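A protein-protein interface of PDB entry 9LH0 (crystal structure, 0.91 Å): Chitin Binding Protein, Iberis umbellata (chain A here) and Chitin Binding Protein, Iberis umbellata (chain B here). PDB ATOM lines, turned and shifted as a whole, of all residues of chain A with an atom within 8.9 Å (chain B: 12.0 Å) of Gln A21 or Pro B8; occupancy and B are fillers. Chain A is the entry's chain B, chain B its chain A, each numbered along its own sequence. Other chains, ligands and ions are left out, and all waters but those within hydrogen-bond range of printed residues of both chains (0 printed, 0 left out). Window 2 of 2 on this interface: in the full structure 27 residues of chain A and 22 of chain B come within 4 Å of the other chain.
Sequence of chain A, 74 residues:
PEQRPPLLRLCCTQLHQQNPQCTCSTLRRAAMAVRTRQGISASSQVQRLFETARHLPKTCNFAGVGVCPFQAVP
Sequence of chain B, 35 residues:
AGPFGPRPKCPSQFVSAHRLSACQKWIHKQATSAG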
ATOM      1  N   LEU A  15      33.057 -26.055 -29.894  1.00  0.00           N
ATOM      2  CA  LEU A  15      32.193 -25.091 -29.214  1.00  0.00           C
ATOM      3  C   LEU A  15      30.855 -25.714 -28.836  1.00  0.00           C
ATOM      4  O   LEU A  15      30.291 -25.395 -27.781  1.00  0.00           O
ATOM      5  CB  LEU A  15      31.975 -23.859 -30.095  1.00  0.00           C
ATOM      6  CG  LEU A  15      33.115 -22.859 -30.136  1.00  0.00           C
ATOM      7  CD1 LEU A  15      32.854 -21.783 -31.180  1.00  0.00           C
ATOM      8  CD2 LEU A  15      33.286 -22.260 -28.744  1.00  0.00           C
ATOM      9  N   GLN A  18      29.973 -27.196 -25.399  1.00  0.00           N
ATOM     10  CA  GLN A  18      29.795 -26.295 -24.273  1.00  0.00           C
ATOM     11  C   GLN A  18      28.384 -25.718 -24.268  1.00  0.00           C
ATOM     12  O   GLN A  18      27.730 -25.620 -25.311  1.00  0.00           O
ATOM     13  CB  GLN A  18      30.816 -25.159 -24.349  1.00  0.00           C
ATOM     14  CG  GLN A  18      32.246 -25.647 -24.480  1.00  0.00           C
ATOM     15  CD  GLN A  18      33.242 -24.533 -24.354  1.00  0.00           C
ATOM     16  OE1 GLN A  18      34.311 -24.689 -23.772  1.00  0.00           O
ATOM     17  NE2 GLN A  18      32.895 -23.390 -24.909  1.00  0.00           N
ATOM     18  N   ASN A  19      27.920 -25.324 -23.081  1.00  0.00           N
ATOM     19  CA  ASN A  19      26.650 -24.630 -22.981  1.00  0.00           C
ATOM     20  C   ASN A  19      26.778 -23.205 -23.522  1.00  0.00           C
ATOM     21  O   ASN A  19      27.828 -22.572 -23.383  1.00  0.00           O
ATOM     22  CB  ASN A  19      26.199 -24.559 -21.526  1.00  0.00           C
ATOM     23  CG  ASN A  19      25.918 -25.916 -20.934  1.00  0.00           C
ATOM     24  OD1 ASN A  19      26.457 -26.263 -19.893  1.00  0.00           O
ATOM     25  ND2 ASN A  19      25.060 -26.682 -21.577  1.00  0.00           N
ATOM     26  N   PRO A  20      25.698 -22.669 -24.103  1.00  0.00           N
ATOM     27  CA  PRO A  20      25.739 -21.299 -24.646  1.00  0.00           C
ATOM     28  C   PRO A  20      26.288 -20.263 -23.689  1.00  0.00           C
ATOM     29  O   PRO A  20      27.089 -19.416 -24.092  1.00  0.00           O
ATOM     30  CB  PRO A  20      24.269 -21.031 -24.995  1.00  0.00           C
ATOM     31  CG  PRO A  20      23.722 -22.384 -25.317  1.00  0.00           C
ATOM     32  CD  PRO A  20      24.422 -23.342 -24.397  1.00  0.00           C
ATOM     33  N   GLN A  21      25.885 -20.316 -22.428  1.00  0.00           N
ATOM     34  CA  GLN A  21      26.299 -19.318 -21.457  1.00  0.00           C
ATOM     35  C   GLN A  21      27.727 -19.531 -20.951  1.00  0.00           C
ATOM     36  O   GLN A  21      28.196 -18.743 -20.127  1.00  0.00           O
ATOM     37  CB  GLN A  21      25.253 -19.181 -20.340  1.00  0.00           C
ATOM     38  CG  GLN A  21      25.106 -20.378 -19.437  1.00  0.00           C
ATOM     39  CD  GLN A  21      24.176 -21.471 -19.947  1.00  0.00           C
ATOM     40  OE1 GLN A  21      24.043 -21.752 -21.137  1.00  0.00           O
ATOM     41  NE2 GLN A  21      23.562 -22.132 -19.011  1.00  0.00           N
ATOM     42  N   CYS A  22      28.432 -20.556 -21.444  1.00  0.00           N
ATOM     43  CA  CYS A  22      29.869 -20.711 -21.233  1.00  0.00           C
ATOM     44  C   CYS A  22      30.712 -20.296 -22.431  1.00  0.00           C
ATOM     45  O   CYS A  22      31.929 -20.136 -22.282  1.00  0.00           O
ATOM     46  CB  CYS A  22      30.215 -22.173 -20.922  1.00  0.00           C
ATOM     47  SG  CYS A  22      29.683 -22.776 -19.309  1.00  0.00           S
ATOM     48  N   THR A  23      30.110 -20.142 -23.609  1.00  0.00           N
ATOM     49  CA  THR A  23      30.892 -20.030 -24.836  1.00  0.00           C
ATOM     50  C   THR A  23      31.777 -18.778 -24.845  1.00  0.00           C
ATOM     51  O   THR A  23      32.970 -18.861 -25.151  1.00  0.00           O
ATOM     52  CB  THR A  23      29.963 -20.136 -26.054  1.00  0.00           C
ATOM     53  OG1 THR A  23      29.539 -21.503 -26.224  1.00  0.00           O
ATOM     54  CG2 THR A  23      30.652 -19.664 -27.308  1.00  0.00           C
ATOM     55  N   CYS A  24      31.229 -17.615 -24.481  1.00  0.00           N
ATOM     56  CA  CYS A  24      32.033 -16.396 -24.568  1.00  0.00           C
ATOM     57  C   CYS A  24      33.180 -16.394 -23.563  1.00  0.00           C
ATOM     58  O   CYS A  24      34.297 -15.984 -23.894  1.00  0.00           O
ATOM     59  CB  CYS A  24      31.154 -15.156 -24.424  1.00  0.00           C
ATOM     60  SG  CYS A  24      30.044 -14.936 -25.819  1.00  0.00           S
ATOM     61  N   SER A  25      32.925 -16.855 -22.335  1.00  0.00           N
ATOM     62  CA  SER A  25      33.979 -16.913 -21.327  1.00  0.00           C
ATOM     63  C   SER A  25      35.106 -17.837 -21.772  1.00  0.00           C
ATOM     64  O   SER A  25      36.290 -17.508 -21.629  1.00  0.00           O
ATOM     65  CB  SER A  25      33.392 -17.371 -19.989  1.00  0.00           C
ATOM     66  OG  SER A  25      34.384 -17.450 -18.978  1.00  0.00           O
ATOM     67  N   THR A  26      34.757 -18.995 -22.333  1.00  0.00           N
ATOM     68  CA  THR A  26      35.792 -19.929 -22.758  1.00  0.00           C
ATOM     69  C   THR A  26      36.528 -19.442 -24.000  1.00  0.00           C
ATOM     70  O   THR A  26      37.723 -19.713 -24.147  1.00  0.00           O
ATOM     71  CB  THR A  26      35.220 -21.331 -22.982  1.00  0.00           C
ATOM     72  OG1 THR A  26      34.234 -21.299 -24.018  1.00  0.00           O
ATOM     73  CG2 THR A  26      34.613 -21.886 -21.690  1.00  0.00           C
ATOM     74  N   PHE A  62      25.940 -20.380 -33.885  1.00  0.00           N
ATOM     75  CA  PHE A  62      25.538 -20.629 -32.501  1.00  0.00           C
ATOM     76  C   PHE A  62      24.538 -19.534 -32.137  1.00  0.00           C
ATOM     77  O   PHE A  62      24.844 -18.573 -31.426  1.00  0.00           O
ATOM     78  CB  PHE A  62      26.771 -20.564 -31.606  1.00  0.00           C
ATOM     79  CG  PHE A  62      26.750 -21.516 -30.443  1.00  0.00           C
ATOM     80  CD1 PHE A  62      25.820 -21.379 -29.427  1.00  0.00           C
ATOM     81  CD2 PHE A  62      27.698 -22.522 -30.344  1.00  0.00           C
ATOM     82  CE1 PHE A  62      25.818 -22.248 -28.348  1.00  0.00           C
ATOM     83  CE2 PHE A  62      27.702 -23.393 -29.270  1.00  0.00           C
ATOM     84  CZ  PHE A  62      26.759 -23.256 -28.271  1.00  0.00           C
ATOM     85  N   GLY A  64      21.993 -19.041 -30.251  1.00  0.00           N
ATOM     86  CA  GLY A  64      21.651 -18.666 -28.891  1.00  0.00           C
ATOM     87  C   GLY A  64      22.636 -17.750 -28.196  1.00  0.00           C
ATOM     88  O   GLY A  64      22.380 -17.349 -27.057  1.00  0.00           O
ATOM     89  N   VAL A  65      23.750 -17.398 -28.841  1.00  0.00           N
ATOM     90  CA  VAL A  65      24.809 -16.599 -28.234  1.00  0.00           C
ATOM     91  C   VAL A  65      25.020 -15.286 -28.978  1.00  0.00           C
ATOM     92  O   VAL A  65      25.056 -14.212 -28.369  1.00  0.00           O
ATOM     93  CB  VAL A  65      26.132 -17.394 -28.130  1.00  0.00           C
ATOM     94  CG1 VAL A  65      27.263 -16.501 -27.638  1.00  0.00           C
ATOM     95  CG2 VAL A  65      25.957 -18.591 -27.215  1.00  0.00           C
ATOM     96  N   CYS A  68      30.098 -12.246 -28.941  1.00  0.00           N
ATOM     97  CA  CYS A  68      30.438 -12.000 -27.551  1.00  0.00           C
ATOM     98  C   CYS A  68      30.789 -10.533 -27.333  1.00  0.00           C
ATOM     99  O   CYS A  68      31.389  -9.900 -28.200  1.00  0.00           O
ATOM    100  CB  CYS A  68      31.655 -12.823 -27.186  1.00  0.00           C
ATOM    101  SG  CYS A  68      31.345 -14.602 -27.354  1.00  0.00           S
ATOM    102  N   ALA B   1      16.942 -22.317 -10.430  1.00  0.00           N
ATOM    103  CA  ALA B   1      18.246 -22.777  -9.968  1.00  0.00           C
ATOM    104  C   ALA B   1      18.109 -23.599  -8.688  1.00  0.00           C
ATOM    105  O   ALA B   1      17.449 -23.180  -7.736  1.00  0.00           O
ATOM    106  CB  ALA B   1      19.177 -21.594  -9.748  1.00  0.00           C
ATOM    107  N   GLY B   2      18.737 -24.770  -8.668  1.00  0.00           N
ATOM    108  CA  GLY B   2      18.650 -25.656  -7.533  1.00  0.00           C
ATOM    109  C   GLY B   2      19.857 -26.562  -7.409  1.00  0.00           C
ATOM    110  O   GLY B   2      20.705 -26.633  -8.308  1.00  0.00           O
ATOM    111  N   PRO B   3      19.948 -27.287  -6.291  1.00  0.00           N
ATOM    112  CA  PRO B   3      21.122 -28.149  -6.067  1.00  0.00           C
ATOM    113  C   PRO B   3      21.276 -29.251  -7.095  1.00  0.00           C
ATOM    114  O   PRO B   3      22.385 -29.768  -7.270  1.00  0.00           O
ATOM    115  CB  PRO B   3      20.881 -28.719  -4.662  1.00  0.00           C
ATOM    116  CG  PRO B   3      19.400 -28.638  -4.472  1.00  0.00           C
ATOM    117  CD  PRO B   3      18.960 -27.400  -5.205  1.00  0.00           C
ATOM    118  N   PHE B   4      20.200 -29.630  -7.784  1.00  0.00           N
ATOM    119  CA  PHE B   4      20.248 -30.703  -8.767  1.00  0.00           C
ATOM    120  C   PHE B   4      19.960 -30.206 -10.178  1.00  0.00           C
ATOM    121  O   PHE B   4      19.606 -30.998 -11.052  1.00  0.00           O
ATOM    122  CB  PHE B   4      19.320 -31.849  -8.349  1.00  0.00           C
ATOM    123  CG  PHE B   4      19.636 -32.400  -6.983  1.00  0.00           C
ATOM    124  CD1 PHE B   4      20.665 -33.311  -6.816  1.00  0.00           C
ATOM    125  CD2 PHE B   4      18.935 -31.977  -5.863  1.00  0.00           C
ATOM    126  CE1 PHE B   4      20.972 -33.811  -5.560  1.00  0.00           C
ATOM    127  CE2 PHE B   4      19.238 -32.475  -4.609  1.00  0.00           C
ATOM    128  CZ  PHE B   4      20.258 -33.391  -4.459  1.00  0.00           C
ATOM    129  N   GLY B   5      20.120 -28.900 -10.420  1.00  0.00           N
ATOM    130  CA  GLY B   5      19.985 -28.355 -11.742  1.00  0.00           C
ATOM    131  C   GLY B   5      21.161 -28.736 -12.628  1.00  0.00           C
ATOM    132  O   GLY B   5      22.101 -29.417 -12.201  1.00  0.00           O
ATOM    133  N   PRO B   6      21.120 -28.284 -13.884  1.00  0.00           N
ATOM    134  CA  PRO B   6      22.216 -28.628 -14.805  1.00  0.00           C
ATOM    135  C   PRO B   6      23.576 -28.150 -14.328  1.00  0.00           C
ATOM    136  O   PRO B   6      24.577 -28.845 -14.549  1.00  0.00           O
ATOM    137  CB  PRO B   6      21.772 -28.008 -16.135  1.00  0.00           C
ATOM    138  CG  PRO B   6      20.730 -26.997 -15.775  1.00  0.00           C
ATOM    139  CD  PRO B   6      20.048 -27.534 -14.553  1.00  0.00           C
ATOM    140  N   ARG B   7      23.639 -26.987 -13.683  1.00  0.00           N
ATOM    141  CA  ARG B   7      24.856 -26.487 -13.052  1.00  0.00           C
ATOM    142  C   ARG B   7      26.089 -26.537 -13.958  1.00  0.00           C
ATOM    143  O   ARG B   7      27.060 -27.244 -13.661  1.00  0.00           O
ATOM    144  CB  ARG B   7      25.120 -27.180 -11.724  1.00  0.00           C
ATOM    145  CG  ARG B   7      24.001 -26.949 -10.732  1.00  0.00           C
ATOM    146  CD  ARG B   7      24.327 -27.501  -9.369  1.00  0.00           C
ATOM    147  NE  ARG B   7      23.774 -26.620  -8.352  1.00  0.00           N
ATOM    148  CZ  ARG B   7      24.334 -26.381  -7.176  1.00  0.00           C
ATOM    149  NH1 ARG B   7      25.450 -26.986  -6.805  1.00  0.00           N
ATOM    150  NH2 ARG B   7      23.768 -25.499  -6.359  1.00  0.00           N
ATOM    151  N   PRO B   8      26.083 -25.795 -15.064  1.00  0.00           N
ATOM    152  CA  PRO B   8      27.247 -25.785 -15.960  1.00  0.00           C
ATOM    153  C   PRO B   8      28.509 -25.370 -15.226  1.00  0.00           C
ATOM    154  O   PRO B   8      28.502 -24.422 -14.443  1.00  0.00           O
ATOM    155  CB  PRO B   8      26.872 -24.733 -17.012  1.00  0.00           C
ATOM    156  CG  PRO B   8      25.395 -24.614 -16.950  1.00  0.00           C
ATOM    157  CD  PRO B   8      25.024 -24.884 -15.524  1.00  0.00           C
ATOM    158  N   LYS B   9      29.612 -26.054 -15.524  1.00  0.00           N
ATOM    159  CA  LYS B   9      30.935 -25.728 -14.991  1.00  0.00           C
ATOM    160  C   LYS B   9      31.794 -25.366 -16.197  1.00  0.00           C
ATOM    161  O   LYS B   9      32.372 -26.239 -16.850  1.00  0.00           O
ATOM    162  CB  LYS B   9      31.531 -26.904 -14.217  1.00  0.00           C
ATOM    163  CG  LYS B   9      30.642 -27.462 -13.120  1.00  0.00           C
ATOM    164  CD  LYS B   9      30.239 -26.409 -12.109  1.00  0.00           C
ATOM    165  CE  LYS B   9      29.325 -27.012 -11.055  1.00  0.00           C
ATOM    166  NZ  LYS B   9      28.698 -25.976 -10.198  1.00  0.00           N
ATOM    167  N   CYS B  10      31.873 -24.072 -16.496  1.00  0.00           N
ATOM    168  CA  CYS B  10      32.541 -23.655 -17.725  1.00  0.00           C
ATOM    169  C   CYS B  10      33.999 -24.102 -17.826  1.00  0.00           C
ATOM    170  O   CYS B  10      34.402 -24.535 -18.920  1.00  0.00           O
ATOM    171  CB  CYS B  10      32.368 -22.147 -17.959  1.00  0.00           C
ATOM    172  SG  CYS B  10      30.653 -21.554 -18.010  1.00  0.00           S
ATOM    173  N   PRO B  11      34.826 -24.040 -16.771  1.00  0.00           N
ATOM    174  CA  PRO B  11      36.219 -24.499 -16.935  1.00  0.00           C
ATOM    175  C   PRO B  11      36.338 -25.981 -17.251  1.00  0.00           C
ATOM    176  O   PRO B  11      37.219 -26.384 -18.021  1.00  0.00           O
ATOM    177  CB  PRO B  11      36.873 -24.137 -15.592  1.00  0.00           C
ATOM    178  CG  PRO B  11      36.024 -23.048 -15.037  1.00  0.00           C
ATOM    179  CD  PRO B  11      34.628 -23.371 -15.472  1.00  0.00           C
ATOM    180  N   SER B  12      35.473 -26.808 -16.660  1.00  0.00           N
ATOM    181  CA  SER B  12      35.475 -28.233 -16.969  1.00  0.00           C
ATOM    182  C   SER B  12      35.025 -28.481 -18.402  1.00  0.00           C
ATOM    183  O   SER B  12      35.592 -29.328 -19.100  1.00  0.00           O
ATOM    184  CB  SER B  12      34.579 -28.976 -15.975  1.00  0.00           C
ATOM    185  OG  SER B  12      34.591 -30.373 -16.208  1.00  0.00           O
ATOM    186  N   GLN B  13      34.013 -27.742 -18.865  1.00  0.00           N
ATOM    187  CA  GLN B  13      33.584 -27.875 -20.252  1.00  0.00           C
ATOM    188  C   GLN B  13      34.706 -27.497 -21.204  1.00  0.00           C
ATOM    189  O   GLN B  13      34.894 -28.141 -22.238  1.00  0.00           O
ATOM    190  CB  GLN B  13      32.347 -27.017 -20.511  1.00  0.00           C
ATOM    191  CG  GLN B  13      31.153 -27.469 -19.717  1.00  0.00           C
ATOM    192  CD  GLN B  13      29.894 -26.697 -20.029  1.00  0.00           C
ATOM    193  OE1 GLN B  13      29.826 -25.903 -20.963  1.00  0.00           O
ATOM    194  NE2 GLN B  13      28.881 -26.929 -19.232  1.00  0.00           N
ATOM    195  N   PHE B  14      35.469 -26.463 -20.854  1.00  0.00           N
ATOM    196  CA  PHE B  14      36.578 -26.015 -21.689  1.00  0.00           C
ATOM    197  C   PHE B  14      37.620 -27.110 -21.848  1.00  0.00           C
ATOM    198  O   PHE B  14      38.057 -27.409 -22.965  1.00  0.00           O
ATOM    199  CB  PHE B  14      37.195 -24.773 -21.051  1.00  0.00           C
ATOM    200  CG  PHE B  14      38.321 -24.154 -21.840  1.00  0.00           C
ATOM    201  CD1 PHE B  14      38.109 -23.626 -23.103  1.00  0.00           C
ATOM    202  CD2 PHE B  14      39.590 -24.072 -21.292  1.00  0.00           C
ATOM    203  CE1 PHE B  14      39.146 -23.026 -23.802  1.00  0.00           C
ATOM    204  CE2 PHE B  14      40.631 -23.488 -21.990  1.00  0.00           C
ATOM    205  CZ  PHE B  14      40.407 -22.959 -23.244  1.00  0.00           C
ATOM    206  N   VAL B  15      38.035 -27.727 -20.740  1.00  0.00           N
ATOM    207  CA  VAL B  15      39.050 -28.770 -20.838  1.00  0.00           C
ATOM    208  C   VAL B  15      38.499 -30.003 -21.547  1.00  0.00           C
ATOM    209  O   VAL B  15      39.201 -30.638 -22.342  1.00  0.00           O
ATOM    210  CB  VAL B  15      39.690 -29.080 -19.470  1.00  0.00           C
ATOM    211  CG1 VAL B  15      40.494 -27.888 -18.982  1.00  0.00           C
ATOM    212  CG2 VAL B  15      38.638 -29.447 -18.454  1.00  0.00           C
ATOM    213  N   SER B  16      37.225 -30.330 -21.313  1.00  0.00           N
ATOM    214  CA  SER B  16      36.616 -31.465 -22.004  1.00  0.00           C
ATOM    215  C   SER B  16      36.541 -31.233 -23.510  1.00  0.00           C
ATOM    216  O   SER B  16      36.627 -32.188 -24.293  1.00  0.00           O
ATOM    217  CB  SER B  16      35.225 -31.751 -21.429  1.00  0.00           C
ATOM    218  OG  SER B  16      35.291 -32.140 -20.065  1.00  0.00           O
ATOM    219  N   LEU B  20      39.253 -25.925 -26.674  1.00  0.00           N
ATOM    220  CA  LEU B  20      38.890 -25.322 -27.950  1.00  0.00           C
ATOM    221  C   LEU B  20      40.103 -25.226 -28.879  1.00  0.00           C
ATOM    222  O   LEU B  20      40.306 -24.228 -29.563  1.00  0.00           O
ATOM    223  CB  LEU B  20      38.201 -23.963 -27.767  1.00  0.00           C
ATOM    224  CG  LEU B  20      36.993 -23.947 -26.831  1.00  0.00           C
ATOM    225  CD1 LEU B  20      36.481 -22.513 -26.685  1.00  0.00           C
ATOM    226  CD2 LEU B  20      35.900 -24.878 -27.325  1.00  0.00           C
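Of the printed residues of chain B, Gln A18 touches Gln B13 (3.3 Å), Phe B14 (3.4 Å) and Leu B20 (3.9 Å).
No residue of chain B comes within 4 Å of Pro A20.
Gln A21 touches just one residue of chain B: Pro B8 (3.7 Å).
Cys A22 touches just these residues of chain B: Cys B10 (2.0 Å) and Gln B13 (3.5 Å).
No residue of chain B comes within 4 Å of Thr A23.
No residue of chain B comes within 4 Å of Cys A24.
Of chain A, only Asn A19 (3.3 Å) and Gln A21 (3.7 Å) come within 4 Å of Pro B8.
No residue of chain A comes within 4 Å of Lys B9.
Printed residues of chain A within 4 Å of Cys B10: Cys A22 and Thr A26.
Pro B11 touches none of the printed residues of chain A.
The nearest residue of chain B that does not touch Gln A21 is Cys B10 (4.3 Å).
The nearest residue of chain A that does not touch Pro B8 is Cys A22 (4.1 Å).
NE2 of Gln A18 is in hydrogen-bond range of OG1 of Thr A26 (2.6 Å).
O of Asn A19 is in hydrogen-bond range of OG1 of Thr A23 (3.5 Å).
The backbone carbonyl oxygen of Cys A22 sits at hydrogen-bond distance from the side-chain hydroxyl of Thr A26.
The backbone carbonyl oxygen (O) of Thr A23 is in hydrogen-bond range of the side-chain hydroxyl (OG1) of Thr A26, at 3.0 Å.
The side-chain sulfur (SG) of Cys A24 forms a disulfide with the side-chain sulfur (SG) of Cys A68 (2.0 Å).
Hydrophobic or aromatic side chains of chain B within 4 Å of the printed part of chain A: Pro B8, Phe B14 and Leu B20.
Printed residues of chain A that touch a printed residue of chain B: Leu A15, Gln A18, Asn A19, Gln A21, Cys A22 and Thr A26.
Hydrophobic or aromatic side chains of chain A that line the printed part of chain B: Leu A15.
The side-chain sulfur (SG) of Cys B10 is disulfide-bonded to the side-chain sulfur (SG) of Cys A22.
The side-chain amide oxygen of Asn A19 is in hydrogen-bond range of the side-chain amide nitrogen of Gln B13, 2.6 Å away.
The side-chain amide oxygen (OE1) of Gln B13 lies close to the side-chain sulfur (SG) of Cys A22 (3.5 Å).
CD1 of Leu B20 touches CD2 of Leu A15, 3.8 Å away.
Gln A18 touches Gln B13 (CA to OE1, 3.3 Å).
OE1 of Gln A18 touches CA of Phe B14 (3.4 Å).
Leu B20 touches Gln A18.
Asn A19 touches Pro B8 (OD1 to CB, 3.3 Å).
Gln A21 touches Pro B8.
CG2 of Thr A26 touches O of Cys B10 (3.8 Å).
Thr A26 touches Phe B14.
Thr A26 touches Leu B20.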
